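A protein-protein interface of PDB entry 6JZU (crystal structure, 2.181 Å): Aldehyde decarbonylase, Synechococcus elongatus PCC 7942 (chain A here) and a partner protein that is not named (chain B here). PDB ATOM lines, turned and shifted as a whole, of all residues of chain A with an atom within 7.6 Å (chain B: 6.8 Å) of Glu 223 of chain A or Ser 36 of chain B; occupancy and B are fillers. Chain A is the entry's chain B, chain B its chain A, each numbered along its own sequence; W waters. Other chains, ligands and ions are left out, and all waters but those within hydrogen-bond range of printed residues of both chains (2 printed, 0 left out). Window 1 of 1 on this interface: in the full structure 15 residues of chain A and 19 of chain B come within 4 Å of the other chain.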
ATOM      1  N   ALA A 143     -27.948   1.528 -25.353  1.00  0.00           N
ATOM      2  CA  ALA A 143     -27.880   0.140 -24.920  1.00  0.00           C
ATOM      3  C   ALA A 143     -29.152  -0.610 -25.300  1.00  0.00           C
ATOM      4  O   ALA A 143     -29.098  -1.679 -25.923  1.00  0.00           O
ATOM      5  CB  ALA A 143     -27.650   0.078 -23.411  1.00  0.00           C
ATOM      6  N   ILE A 147     -29.335  -3.713 -28.261  1.00  0.00           N
ATOM      7  CA  ILE A 147     -29.741  -5.049 -27.857  1.00  0.00           C
ATOM      8  C   ILE A 147     -31.042  -5.438 -28.535  1.00  0.00           C
ATOM      9  O   ILE A 147     -31.308  -6.624 -28.760  1.00  0.00           O
ATOM     10  CB  ILE A 147     -29.870  -5.098 -26.321  1.00  0.00           C
ATOM     11  CG1 ILE A 147     -28.538  -4.734 -25.651  1.00  0.00           C
ATOM     12  CG2 ILE A 147     -30.355  -6.452 -25.853  1.00  0.00           C
ATOM     13  CD1 ILE A 147     -27.339  -5.357 -26.284  1.00  0.00           C
ATOM     14  N   TRP A 201     -29.888   1.178 -12.610  1.00  0.00           N
ATOM     15  CA  TRP A 201     -29.830  -0.219 -12.187  1.00  0.00           C
ATOM     16  C   TRP A 201     -31.183  -0.692 -11.678  1.00  0.00           C
ATOM     17  O   TRP A 201     -31.615  -1.802 -12.000  1.00  0.00           O
ATOM     18  CB  TRP A 201     -28.750  -0.424 -11.119  1.00  0.00           C
ATOM     19  CG  TRP A 201     -27.414   0.172 -11.472  1.00  0.00           C
ATOM     20  CD1 TRP A 201     -26.612   0.921 -10.655  1.00  0.00           C
ATOM     21  CD2 TRP A 201     -26.729   0.086 -12.733  1.00  0.00           C
ATOM     22  NE1 TRP A 201     -25.474   1.304 -11.325  1.00  0.00           N
ATOM     23  CE2 TRP A 201     -25.520   0.802 -12.600  1.00  0.00           C
ATOM     24  CE3 TRP A 201     -27.017  -0.532 -13.958  1.00  0.00           C
ATOM     25  CZ2 TRP A 201     -24.603   0.922 -13.646  1.00  0.00           C
ATOM     26  CZ3 TRP A 201     -26.112  -0.404 -14.998  1.00  0.00           C
ATOM     27  CH2 TRP A 201     -24.916   0.316 -14.834  1.00  0.00           C
ATOM     28  N   LEU A 204     -33.417  -1.162 -14.793  1.00  0.00           N
ATOM     29  CA  LEU A 204     -33.106  -2.381 -15.537  1.00  0.00           C
ATOM     30  C   LEU A 204     -33.591  -3.618 -14.805  1.00  0.00           C
ATOM     31  O   LEU A 204     -33.935  -4.618 -15.442  1.00  0.00           O
ATOM     32  CB  LEU A 204     -31.603  -2.490 -15.805  1.00  0.00           C
ATOM     33  CG  LEU A 204     -31.136  -1.716 -17.046  1.00  0.00           C
ATOM     34  CD1 LEU A 204     -29.622  -1.747 -17.203  1.00  0.00           C
ATOM     35  CD2 LEU A 204     -31.820  -2.243 -18.303  1.00  0.00           C
ATOM     36  N   GLU A 217     -31.188  -9.932 -23.053  1.00  0.00           N
ATOM     37  CA  GLU A 217     -30.651 -10.326 -21.762  1.00  0.00           C
ATOM     38  C   GLU A 217     -30.213  -9.106 -20.959  1.00  0.00           C
ATOM     39  O   GLU A 217     -29.630  -8.158 -21.495  1.00  0.00           O
ATOM     40  CB  GLU A 217     -29.483 -11.296 -21.941  1.00  0.00           C
ATOM     41  N   ARG A 218     -30.509  -9.151 -19.662  1.00  0.00           N
ATOM     42  CA  ARG A 218     -30.066  -8.116 -18.739  1.00  0.00           C
ATOM     43  C   ARG A 218     -28.548  -7.922 -18.816  1.00  0.00           C
ATOM     44  O   ARG A 218     -28.051  -6.792 -18.927  1.00  0.00           O
ATOM     45  CB  ARG A 218     -30.512  -8.510 -17.327  1.00  0.00           C
ATOM     46  CG  ARG A 218     -30.252  -7.464 -16.275  1.00  0.00           C
ATOM     47  CD  ARG A 218     -30.566  -7.977 -14.892  1.00  0.00           C
ATOM     48  NE  ARG A 218     -30.166  -7.006 -13.876  1.00  0.00           N
ATOM     49  CZ  ARG A 218     -28.907  -6.819 -13.479  1.00  0.00           C
ATOM     50  NH1 ARG A 218     -27.922  -7.542 -14.010  1.00  0.00           N
ATOM     51  NH2 ARG A 218     -28.631  -5.910 -12.552  1.00  0.00           N
ATOM     52  N   GLU A 219     -27.802  -9.031 -18.815  1.00  0.00           N
ATOM     53  CA  GLU A 219     -26.343  -8.971 -18.838  1.00  0.00           C
ATOM     54  C   GLU A 219     -25.839  -8.129 -20.003  1.00  0.00           C
ATOM     55  O   GLU A 219     -24.965  -7.270 -19.828  1.00  0.00           O
ATOM     56  CB  GLU A 219     -25.775 -10.395 -18.901  1.00  0.00           C
ATOM     57  CG  GLU A 219     -24.277 -10.502 -19.197  1.00  0.00           C
ATOM     58  CD  GLU A 219     -23.832 -11.963 -19.413  1.00  0.00           C
ATOM     59  OE1 GLU A 219     -24.227 -12.838 -18.599  1.00  0.00           O
ATOM     60  OE2 GLU A 219     -23.101 -12.235 -20.401  1.00  0.00           O
ATOM     61  N   SER A 220     -26.408  -8.328 -21.194  1.00  0.00           N
ATOM     62  CA  SER A 220     -25.979  -7.538 -22.343  1.00  0.00           C
ATOM     63  C   SER A 220     -26.406  -6.078 -22.223  1.00  0.00           C
ATOM     64  O   SER A 220     -25.709  -5.181 -22.729  1.00  0.00           O
ATOM     65  CB  SER A 220     -26.544  -8.142 -23.626  1.00  0.00           C
ATOM     66  OG  SER A 220     -26.163  -9.498 -23.744  1.00  0.00           O
ATOM     67  N   LEU A 221     -27.553  -5.819 -21.591  1.00  0.00           N
ATOM     68  CA  LEU A 221     -27.990  -4.437 -21.413  1.00  0.00           C
ATOM     69  C   LEU A 221     -27.040  -3.679 -20.501  1.00  0.00           C
ATOM     70  O   LEU A 221     -26.653  -2.553 -20.808  1.00  0.00           O
ATOM     71  CB  LEU A 221     -29.411  -4.400 -20.859  1.00  0.00           C
ATOM     72  CG  LEU A 221     -30.455  -4.868 -21.871  1.00  0.00           C
ATOM     73  CD1 LEU A 221     -31.761  -5.279 -21.178  1.00  0.00           C
ATOM     74  CD2 LEU A 221     -30.686  -3.769 -22.889  1.00  0.00           C
ATOM     75  N   VAL A 222     -26.636  -4.285 -19.384  1.00  0.00           N
ATOM     76  CA  VAL A 222     -25.700  -3.620 -18.471  1.00  0.00           C
ATOM     77  C   VAL A 222     -24.413  -3.266 -19.205  1.00  0.00           C
ATOM     78  O   VAL A 222     -23.923  -2.128 -19.150  1.00  0.00           O
ATOM     79  CB  VAL A 222     -25.418  -4.519 -17.249  1.00  0.00           C
ATOM     80  CG1 VAL A 222     -24.304  -3.911 -16.354  1.00  0.00           C
ATOM     81  CG2 VAL A 222     -26.680  -4.754 -16.452  1.00  0.00           C
ATOM     82  N   GLU A 223     -23.874  -4.241 -19.936  1.00  0.00           N
ATOM     83  CA  GLU A 223     -22.597  -4.083 -20.624  1.00  0.00           C
ATOM     84  C   GLU A 223     -22.656  -2.964 -21.645  1.00  0.00           C
ATOM     85  O   GLU A 223     -21.754  -2.122 -21.716  1.00  0.00           O
ATOM     86  CB  GLU A 223     -22.238  -5.410 -21.298  1.00  0.00           C
ATOM     87  CG  GLU A 223     -20.820  -5.557 -21.794  1.00  0.00           C
ATOM     88  CD  GLU A 223     -20.604  -6.929 -22.449  1.00  0.00           C
ATOM     89  OE1 GLU A 223     -20.221  -7.893 -21.739  1.00  0.00           O
ATOM     90  OE2 GLU A 223     -20.837  -7.039 -23.675  1.00  0.00           O
ATOM     91  N   ASP A 224     -23.710  -2.945 -22.466  1.00  0.00           N
ATOM     92  CA  ASP A 224     -23.806  -1.910 -23.497  1.00  0.00           C
ATOM     93  C   ASP A 224     -23.960  -0.539 -22.877  1.00  0.00           C
ATOM     94  O   ASP A 224     -23.334   0.426 -23.330  1.00  0.00           O
ATOM     95  CB  ASP A 224     -24.956  -2.211 -24.458  1.00  0.00           C
ATOM     96  CG  ASP A 224     -24.521  -3.169 -25.567  1.00  0.00           C
ATOM     97  OD1 ASP A 224     -24.298  -4.372 -25.264  1.00  0.00           O
ATOM     98  OD2 ASP A 224     -24.306  -2.715 -26.717  1.00  0.00           O
ATOM     99  N   PHE A 225     -24.773  -0.431 -21.829  1.00  0.00           N
ATOM    100  CA  PHE A 225     -24.874   0.838 -21.115  1.00  0.00           C
ATOM    101  C   PHE A 225     -23.511   1.283 -20.581  1.00  0.00           C
ATOM    102  O   PHE A 225     -23.090   2.420 -20.788  1.00  0.00           O
ATOM    103  CB  PHE A 225     -25.887   0.728 -19.968  1.00  0.00           C
ATOM    104  CG  PHE A 225     -26.018   1.999 -19.201  1.00  0.00           C
ATOM    105  CD1 PHE A 225     -26.922   2.974 -19.608  1.00  0.00           C
ATOM    106  CD2 PHE A 225     -25.180   2.264 -18.117  1.00  0.00           C
ATOM    107  CE1 PHE A 225     -27.017   4.192 -18.916  1.00  0.00           C
ATOM    108  CE2 PHE A 225     -25.276   3.475 -17.416  1.00  0.00           C
ATOM    109  CZ  PHE A 225     -26.194   4.432 -17.816  1.00  0.00           C
ATOM    110  N   MET A 226     -22.808   0.393 -19.873  1.00  0.00           N
ATOM    111  CA  MET A 226     -21.513   0.771 -19.315  1.00  0.00           C
ATOM    112  C   MET A 226     -20.527   1.163 -20.405  1.00  0.00           C
ATOM    113  O   MET A 226     -19.717   2.081 -20.221  1.00  0.00           O
ATOM    114  CB  MET A 226     -20.963  -0.375 -18.469  1.00  0.00           C
ATOM    115  CG  MET A 226     -21.787  -0.573 -17.193  1.00  0.00           C
ATOM    116  SD  MET A 226     -21.052  -1.699 -16.000  1.00  0.00           S
ATOM    117  CE  MET A 226     -19.543  -0.808 -15.561  1.00  0.00           C
ATOM    118  N   ILE A 227     -20.592   0.494 -21.560  1.00  0.00           N
ATOM    119  CA  ILE A 227     -19.677   0.826 -22.645  1.00  0.00           C
ATOM    120  C   ILE A 227     -19.962   2.231 -23.149  1.00  0.00           C
ATOM    121  O   ILE A 227     -19.056   3.061 -23.244  1.00  0.00           O
ATOM    122  CB  ILE A 227     -19.761  -0.223 -23.773  1.00  0.00           C
ATOM    123  CG1 ILE A 227     -19.028  -1.507 -23.370  1.00  0.00           C
ATOM    124  CG2 ILE A 227     -19.184   0.327 -25.084  1.00  0.00           C
ATOM    125  CD1 ILE A 227     -19.144  -2.629 -24.400  1.00  0.00           C
ATOM    126  N   ALA A 228     -21.231   2.530 -23.449  1.00  0.00           N
ATOM    127  CA  ALA A 228     -21.561   3.843 -24.001  1.00  0.00           C
ATOM    128  C   ALA A 228     -21.384   4.961 -22.971  1.00  0.00           C
ATOM    129  O   ALA A 228     -20.943   6.059 -23.319  1.00  0.00           O
ATOM    130  CB  ALA A 228     -22.991   3.841 -24.536  1.00  0.00           C
ATOM    131  N   TYR A 229     -21.737   4.714 -21.704  1.00  0.00           N
ATOM    132  CA  TYR A 229     -21.600   5.741 -20.658  1.00  0.00           C
ATOM    133  C   TYR A 229     -20.136   6.003 -20.320  1.00  0.00           C
ATOM    134  O   TYR A 229     -19.705   7.153 -20.218  1.00  0.00           O
ATOM    135  CB  TYR A 229     -22.374   5.292 -19.409  1.00  0.00           C
ATOM    136  CG  TYR A 229     -22.573   6.331 -18.311  1.00  0.00           C
ATOM    137  CD1 TYR A 229     -23.246   7.519 -18.566  1.00  0.00           C
ATOM    138  CD2 TYR A 229     -22.151   6.083 -16.998  1.00  0.00           C
ATOM    139  CE1 TYR A 229     -23.475   8.453 -17.569  1.00  0.00           C
ATOM    140  CE2 TYR A 229     -22.384   7.023 -15.974  1.00  0.00           C
ATOM    141  CZ  TYR A 229     -23.038   8.204 -16.276  1.00  0.00           C
ATOM    142  OH  TYR A 229     -23.268   9.154 -15.297  1.00  0.00           O
ATOM    143  N   LEU A 251     -24.111  -0.503  -8.588  1.00  0.00           N
ATOM    144  CA  LEU A 251     -24.203  -1.853  -9.132  1.00  0.00           C
ATOM    145  C   LEU A 251     -23.742  -2.891  -8.110  1.00  0.00           C
ATOM    146  O   LEU A 251     -24.515  -3.296  -7.235  1.00  0.00           O
ATOM    147  CB  LEU A 251     -23.376  -1.962 -10.414  1.00  0.00           C
ATOM    148  CG  LEU A 251     -23.781  -3.029 -11.437  1.00  0.00           C
ATOM    149  CD1 LEU A 251     -25.253  -2.936 -11.797  1.00  0.00           C
ATOM    150  CD2 LEU A 251     -22.928  -2.899 -12.691  1.00  0.00           C
ATOM    151  N   LEU B  31     -18.878 -13.291 -10.625  1.00  0.00           N
ATOM    152  CA  LEU B  31     -18.836 -13.648 -12.037  1.00  0.00           C
ATOM    153  C   LEU B  31     -19.832 -12.843 -12.867  1.00  0.00           C
ATOM    154  O   LEU B  31     -19.521 -12.461 -14.000  1.00  0.00           O
ATOM    155  CB  LEU B  31     -19.114 -15.137 -12.205  1.00  0.00           C
ATOM    156  CG  LEU B  31     -18.841 -15.696 -13.606  1.00  0.00           C
ATOM    157  CD1 LEU B  31     -17.479 -15.257 -14.109  1.00  0.00           C
ATOM    158  CD2 LEU B  31     -18.949 -17.242 -13.625  1.00  0.00           C
ATOM    159  N   GLU B  32     -21.032 -12.575 -12.332  1.00  0.00           N
ATOM    160  CA  GLU B  32     -22.055 -11.873 -13.115  1.00  0.00           C
ATOM    161  C   GLU B  32     -21.619 -10.437 -13.428  1.00  0.00           C
ATOM    162  O   GLU B  32     -21.854  -9.944 -14.534  1.00  0.00           O
ATOM    163  CB  GLU B  32     -23.412 -11.902 -12.391  1.00  0.00           C
ATOM    164  CG  GLU B  32     -23.407 -10.945 -11.195  1.00  0.00           C
ATOM    165  CD  GLU B  32     -22.304 -11.249 -10.191  1.00  0.00           C
ATOM    166  OE1 GLU B  32     -22.067 -12.498  -9.917  1.00  0.00           O
ATOM    167  OE2 GLU B  32     -21.605 -10.262  -9.795  1.00  0.00           O
ATOM    168  N   PHE B  33     -20.912  -9.779 -12.503  1.00  0.00           N
ATOM    169  CA  PHE B  33     -20.422  -8.428 -12.767  1.00  0.00           C
ATOM    170  C   PHE B  33     -19.332  -8.434 -13.833  1.00  0.00           C
ATOM    171  O   PHE B  33     -19.325  -7.598 -14.748  1.00  0.00           O
ATOM    172  CB  PHE B  33     -19.886  -7.763 -11.498  1.00  0.00           C
ATOM    173  CG  PHE B  33     -19.121  -6.502 -11.779  1.00  0.00           C
ATOM    174  CD1 PHE B  33     -19.784  -5.344 -12.134  1.00  0.00           C
ATOM    175  CD2 PHE B  33     -17.734  -6.484 -11.724  1.00  0.00           C
ATOM    176  CE1 PHE B  33     -19.077  -4.174 -12.401  1.00  0.00           C
ATOM    177  CE2 PHE B  33     -17.024  -5.320 -11.993  1.00  0.00           C
ATOM    178  CZ  PHE B  33     -17.699  -4.163 -12.328  1.00  0.00           C
ATOM    179  N   TRP B  34     -18.393  -9.373 -13.727  1.00  0.00           N
ATOM    180  CA  TRP B  34     -17.349  -9.457 -14.740  1.00  0.00           C
ATOM    181  C   TRP B  34     -17.935  -9.792 -16.098  1.00  0.00           C
ATOM    182  O   TRP B  34     -17.415  -9.338 -17.128  1.00  0.00           O
ATOM    183  CB  TRP B  34     -16.289 -10.485 -14.314  1.00  0.00           C
ATOM    184  CG  TRP B  34     -15.458  -9.950 -13.207  1.00  0.00           C
ATOM    185  CD1 TRP B  34     -15.798  -9.888 -11.893  1.00  0.00           C
ATOM    186  CD2 TRP B  34     -14.180  -9.333 -13.325  1.00  0.00           C
ATOM    187  NE1 TRP B  34     -14.793  -9.294 -11.172  1.00  0.00           N
ATOM    188  CE2 TRP B  34     -13.786  -8.938 -12.030  1.00  0.00           C
ATOM    189  CE3 TRP B  34     -13.313  -9.098 -14.398  1.00  0.00           C
ATOM    190  CZ2 TRP B  34     -12.561  -8.318 -11.777  1.00  0.00           C
ATOM    191  CZ3 TRP B  34     -12.101  -8.484 -14.150  1.00  0.00           C
ATOM    192  CH2 TRP B  34     -11.731  -8.103 -12.847  1.00  0.00           C
ATOM    193  N   SER B  35     -19.042 -10.544 -16.117  1.00  0.00           N
ATOM    194  CA  SER B  35     -19.693 -10.930 -17.361  1.00  0.00           C
ATOM    195  C   SER B  35     -20.336  -9.751 -18.077  1.00  0.00           C
ATOM    196  O   SER B  35     -20.587  -9.841 -19.284  1.00  0.00           O
ATOM    197  CB  SER B  35     -20.755 -11.993 -17.085  1.00  0.00           C
ATOM    198  OG  SER B  35     -20.167 -13.175 -16.583  1.00  0.00           O
ATOM    199  N   SER B  36     -20.638  -8.662 -17.370  1.00  0.00           N
ATOM    200  CA  SER B  36     -21.157  -7.468 -18.030  1.00  0.00           C
ATOM    201  C   SER B  36     -20.164  -6.304 -18.030  1.00  0.00           C
ATOM    202  O   SER B  36     -20.501  -5.212 -18.492  1.00  0.00           O
ATOM    203  CB  SER B  36     -22.498  -7.059 -17.400  1.00  0.00           C
ATOM    204  OG  SER B  36     -22.456  -7.152 -15.985  1.00  0.00           O
ATOM    205  N   ALA B  37     -18.928  -6.522 -17.598  1.00  0.00           N
ATOM    206  CA  ALA B  37     -18.010  -5.384 -17.463  1.00  0.00           C
ATOM    207  C   ALA B  37     -17.426  -4.977 -18.817  1.00  0.00           C
ATOM    208  O   ALA B  37     -17.152  -5.832 -19.659  1.00  0.00           O
ATOM    209  CB  ALA B  37     -16.880  -5.720 -16.498  1.00  0.00           C
ATOM    210  N   PRO B  38     -17.209  -3.683 -19.042  1.00  0.00           N
ATOM    211  CA  PRO B  38     -16.633  -3.230 -20.301  1.00  0.00           C
ATOM    212  C   PRO B  38     -15.118  -3.403 -20.304  1.00  0.00           C
ATOM    213  O   PRO B  38     -14.507  -3.558 -19.236  1.00  0.00           O
ATOM    214  CB  PRO B  38     -17.031  -1.748 -20.347  1.00  0.00           C
ATOM    215  CG  PRO B  38     -17.103  -1.348 -18.944  1.00  0.00           C
ATOM    216  CD  PRO B  38     -17.546  -2.557 -18.150  1.00  0.00           C
ATOM    217  N   PRO B  39     -14.491  -3.440 -21.488  1.00  0.00           N
ATOM    218  CA  PRO B  39     -13.022  -3.470 -21.549  1.00  0.00           C
ATOM    219  C   PRO B  39     -12.450  -2.171 -21.003  1.00  0.00           C
ATOM    220  O   PRO B  39     -13.085  -1.125 -21.074  1.00  0.00           O
ATOM    221  CB  PRO B  39     -12.729  -3.606 -23.053  1.00  0.00           C
ATOM    222  CG  PRO B  39     -13.950  -3.008 -23.725  1.00  0.00           C
ATOM    223  CD  PRO B  39     -15.101  -3.424 -22.828  1.00  0.00           C
ATOM    224  N   CYS B  63     -11.595  -8.586 -19.331  1.00  0.00           N
ATOM    225  CA  CYS B  63     -12.500  -9.089 -18.294  1.00  0.00           C
ATOM    226  C   CYS B  63     -13.033 -10.473 -18.617  1.00  0.00           C
ATOM    227  O   CYS B  63     -13.989 -10.934 -17.978  1.00  0.00           O
ATOM    228  CB  CYS B  63     -13.680  -8.139 -18.023  1.00  0.00           C
ATOM    229  SG  CYS B  63     -13.151  -6.469 -17.497  1.00  0.00           S
ATOM    230  N   MET B  68     -15.966 -18.554 -17.039  1.00  0.00           N
ATOM    231  CA  MET B  68     -17.056 -18.374 -17.988  1.00  0.00           C
ATOM    232  C   MET B  68     -17.230 -19.582 -18.904  1.00  0.00           C
ATOM    233  O   MET B  68     -18.357 -19.903 -19.299  1.00  0.00           O
ATOM    234  CB  MET B  68     -16.842 -17.111 -18.814  1.00  0.00           C
ATOM    235  CG  MET B  68     -16.881 -15.852 -17.984  1.00  0.00           C
ATOM    236  SD  MET B  68     -16.380 -14.389 -18.951  1.00  0.00           S
ATOM    237  CE  MET B  68     -16.399 -13.180 -17.627  1.00  0.00           C
ATOM    238  N   ARG B  73     -20.952 -19.918 -20.355  1.00  0.00           N
ATOM    239  CA  ARG B  73     -21.271 -18.569 -20.824  1.00  0.00           C
ATOM    240  C   ARG B  73     -20.536 -18.272 -22.134  1.00  0.00           C
ATOM    241  O   ARG B  73     -19.717 -17.354 -22.244  1.00  0.00           O
ATOM    242  CB  ARG B  73     -20.913 -17.555 -19.749  1.00  0.00           C
ATOM    243  CG  ARG B  73     -21.619 -17.780 -18.418  1.00  0.00           C
ATOM    244  CD  ARG B  73     -21.053 -16.796 -17.390  1.00  0.00           C
ATOM    245  NE  ARG B  73     -21.949 -16.490 -16.275  1.00  0.00           N
ATOM    246  CZ  ARG B  73     -22.742 -15.422 -16.240  1.00  0.00           C
ATOM    247  NH1 ARG B  73     -22.768 -14.581 -17.268  1.00  0.00           N
ATOM    248  NH2 ARG B  73     -23.511 -15.192 -15.186  1.00  0.00           N
ATOM    249  N   THR B  76     -21.167 -14.785 -23.518  1.00  0.00           N
ATOM    250  CA  THR B  76     -20.418 -13.835 -22.703  1.00  0.00           C
ATOM    251  C   THR B  76     -18.957 -13.795 -23.127  1.00  0.00           C
ATOM    252  O   THR B  76     -18.385 -12.724 -23.362  1.00  0.00           O
ATOM    253  CB  THR B  76     -20.522 -14.223 -21.230  1.00  0.00           C
ATOM    254  OG1 THR B  76     -21.882 -14.120 -20.799  1.00  0.00           O
ATOM    255  CG2 THR B  76     -19.628 -13.330 -20.379  1.00  0.00           C
ATOM    256  N   ARG B  79     -18.409 -11.971 -26.413  1.00  0.00           N
ATOM    257  CA  ARG B  79     -18.490 -10.514 -26.281  1.00  0.00           C
ATOM    258  C   ARG B  79     -17.239  -9.926 -25.625  1.00  0.00           C
ATOM    259  O   ARG B  79     -16.801  -8.837 -25.996  1.00  0.00           O
ATOM    260  CB  ARG B  79     -19.736 -10.122 -25.480  1.00  0.00           C
ATOM    261  CG  ARG B  79     -21.073 -10.557 -26.099  1.00  0.00           C
ATOM    262  CD  ARG B  79     -22.266  -9.818 -25.445  1.00  0.00           C
ATOM    263  NE  ARG B  79     -22.007  -9.555 -24.037  1.00  0.00           N
ATOM    264  CZ  ARG B  79     -22.396 -10.337 -23.035  1.00  0.00           C
ATOM    265  NH1 ARG B  79     -23.093 -11.440 -23.280  1.00  0.00           N
ATOM    266  NH2 ARG B  79     -22.079 -10.021 -21.781  1.00  0.00           N
ATOM    267  N   LYS B  80     -16.658 -10.610 -24.628  1.00  0.00           N
ATOM    268  CA  LYS B  80     -15.472 -10.043 -23.980  1.00  0.00           C
ATOM    269  C   LYS B  80     -14.383  -9.798 -25.014  1.00  0.00           C
ATOM    270  O   LYS B  80     -13.752  -8.733 -25.043  1.00  0.00           O
ATOM    271  CB  LYS B  80     -14.950 -10.970 -22.868  1.00  0.00           C
ATOM    272  CG  LYS B  80     -15.922 -11.264 -21.709  1.00  0.00           C
ATOM    273  CD  LYS B  80     -16.244 -10.031 -20.831  1.00  0.00           C
ATOM    274  CE  LYS B  80     -17.609  -9.448 -21.174  1.00  0.00           C
ATOM    275  NZ  LYS B  80     -18.163  -8.418 -20.186  1.00  0.00           N
ATOM    276  N   ASN B  83     -15.504  -7.025 -27.685  1.00  0.00           N
ATOM    277  CA  ASN B  83     -15.503  -5.687 -27.082  1.00  0.00           C
ATOM    278  C   ASN B  83     -14.082  -5.182 -26.864  1.00  0.00           C
ATOM    279  O   ASN B  83     -13.789  -4.001 -27.083  1.00  0.00           O
ATOM    280  CB  ASN B  83     -16.246  -5.709 -25.746  1.00  0.00           C
ATOM    281  CG  ASN B  83     -17.732  -5.979 -25.905  1.00  0.00           C
ATOM    282  OD1 ASN B  83     -18.312  -5.712 -26.956  1.00  0.00           O
ATOM    283  ND2 ASN B  83     -18.352  -6.503 -24.855  1.00  0.00           N
ATOM    284  N   ARG B 118     -21.033  -3.233 -32.620  1.00  0.00           N
ATOM    285  CA  ARG B 118     -21.716  -1.945 -32.549  1.00  0.00           C
ATOM    286  C   ARG B 118     -21.405  -1.134 -33.800  1.00  0.00           C
ATOM    287  O   ARG B 118     -21.621  -1.614 -34.917  1.00  0.00           O
ATOM    288  CB  ARG B 118     -21.337  -1.213 -31.263  1.00  0.00           C
ATOM    289  CG  ARG B 118     -22.073  -1.807 -30.063  1.00  0.00           C
ATOM    290  CD  ARG B 118     -21.424  -1.481 -28.714  1.00  0.00           C
ATOM    291  NE  ARG B 118     -21.661  -2.579 -27.778  1.00  0.00           N
ATOM    292  CZ  ARG B 118     -20.743  -3.466 -27.420  1.00  0.00           C
ATOM    293  NH1 ARG B 118     -19.494  -3.358 -27.878  1.00  0.00           N
ATOM    294  NH2 ARG B 118     -21.064  -4.438 -26.582  1.00  0.00           N
HETATM  295  O   HOH W   1     -24.947 -12.150 -15.642  1.00  0.00           O
HETATM  296  O   HOH W   2     -24.984 -11.803 -25.455  1.00  0.00           O
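Glu 223 of chain A touches six residues of chain B. Ser 36 of chain B touches just these residues of chain A: Glu 219 (3.5 Å), Val 222 (3.7 Å) and Glu 223 (3.2 Å). Printed residues of chain B within 4 Å of Glu 219 of chain A: Ser 35, Ser 36, Arg 73, Thr 76 and Arg 79. Of the printed residues of chain A, Ser 35 of chain B touches Glu 219 (3.6 Å) and Glu 223 (3.2 Å). The nearest residue of chain B that does not touch Glu 223 of chain A is Ala 37 of chain B (4.2 Å). The nearest printed residue of chain B that does not touch Asp 224 of chain A is Ser 36 of chain B (5.6 Å).
Water W2 bridges NH1 of Arg 79 of chain B (2.9 Å) and OG of Ser 220 of chain A (3.1 Å). Water W1 bridges OE1 of Glu 219 of chain A and NH2 of Arg 73 of chain B.
The backbone carbonyl oxygen (O) of Leu 31 of chain B is in hydrogen-bond range of the side-chain hydroxyl (OG) of Ser 35 of chain B, at 2.8 Å. NZ of Lys 80 of chain B is in hydrogen-bond range of O of Trp 34 of chain B. NH1 of Arg 73 of chain B lies within hydrogen-bond range of OG of Ser 35 of chain B (3.0 Å). The guanidinium group (NH2) of Arg 79 of chain B is in hydrogen-bond range of the backbone carbonyl oxygen (O) of Ser 35 of chain B, 2.9 Å away. O of Ala 37 of chain B sits at hydrogen-bond distance from NZ of Lys 80 of chain B (2.8 Å). The side-chain sulfur (SG) of Cys 63 of chain B lies within hydrogen-bond range of the backbone carbonyl oxygen (O) of Pro 38 of chain B, at 3.7 Å.
Printed residues of chain A that touch a printed residue of chain B: Glu 219, Ser 220, Val 222, Glu 223, Asp 224, Met 226 and Ile 227. Hydrophobic or aromatic side chains of chain A that line the printed part of chain B: Val 222, Met 226 and Ile 227. Along chain A the printed residues that touch a printed residue of chain B span positions 219 to 227. Hydrophobic or aromatic side chains of chain B within 4 Å of the printed part of chain A: Pro 38. Among the printed residues, Asp or Glu carboxylates within 4 Å of a Lys or Arg side-chain nitrogen of the other chain: Glu 219 of chain A with Arg 73 of chain B, Glu 219 of chain A with Arg 79 of chain B, Glu 223 of chain A with Arg 79 of chain B, Glu 223 of chain A with Lys 80 of chain B, Glu 223 of chain A with Arg 118 of chain B and Asp 224 of chain A with Arg 118 of chain B.
Among the printed residues, merely in contact across the chains: Glu 219 of chain A with Ser 35 of chain B (3.6 Å), Glu 219 of chain A with Ser 36 of chain B (3.5 Å), Ser 220 of chain A with Arg 79 of chain B (3.7 Å), Val 222 of chain A with Ser 36 of chain B (3.7 Å), Glu 223 of chain A with Ser 36 of chain B (3.2 Å), Met 226 of chain A with Pro 38 of chain B (3.7 Å), Ile 227 of chain A with Pro 38 of chain B (3.6 Å), Ile 227 of chain A with Asn 83 of chain B (3.9 Å) and Ile 227 of chain A with Arg 118 of chain B (3.4 Å).
NH1 of Arg 73 of chain B is in salt-bridge range of OE1 of Glu 219 of chain A (2.6 Å). The side-chain hydroxyl (OG1) of Thr 76 of chain B lies close to the side-chain carboxylate (OE1) of Glu 219 of chain A, at 3.5 Å. The guanidinium group of Arg 79 of chain B lies within salt-bridge range of the side-chain carboxylate of Glu 219 of chain A (2.8 Å). The guanidinium group of Arg 79 of chain B is in salt-bridge range of the side-chain carboxylate of Glu 223 of chain A, 2.8 Å away. OE1 of Glu 223 of chain A lies within salt-bridge range of NZ of Lys 80 of chain B, at 2.6 Å. The side-chain amide nitrogen (ND2) of Asn 83 of chain B is in hydrogen-bond range of the side-chain carboxylate (OE2) of Glu 223 of chain A. The guanidinium group (NH2) of Arg 118 of chain B is in salt-bridge range of the side-chain carboxylate (OE2) of Glu 223 of chain A, at 3.9 Å. The guanidinium group (NE) of Arg 118 of chain B is in salt-bridge range of the side-chain carboxylate (OD2) of Asp 224 of chain A, at 2.9 Å. OE1 of Glu 223 of chain A sits close to O of Ser 35 of chain B, 3.2 Å away.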
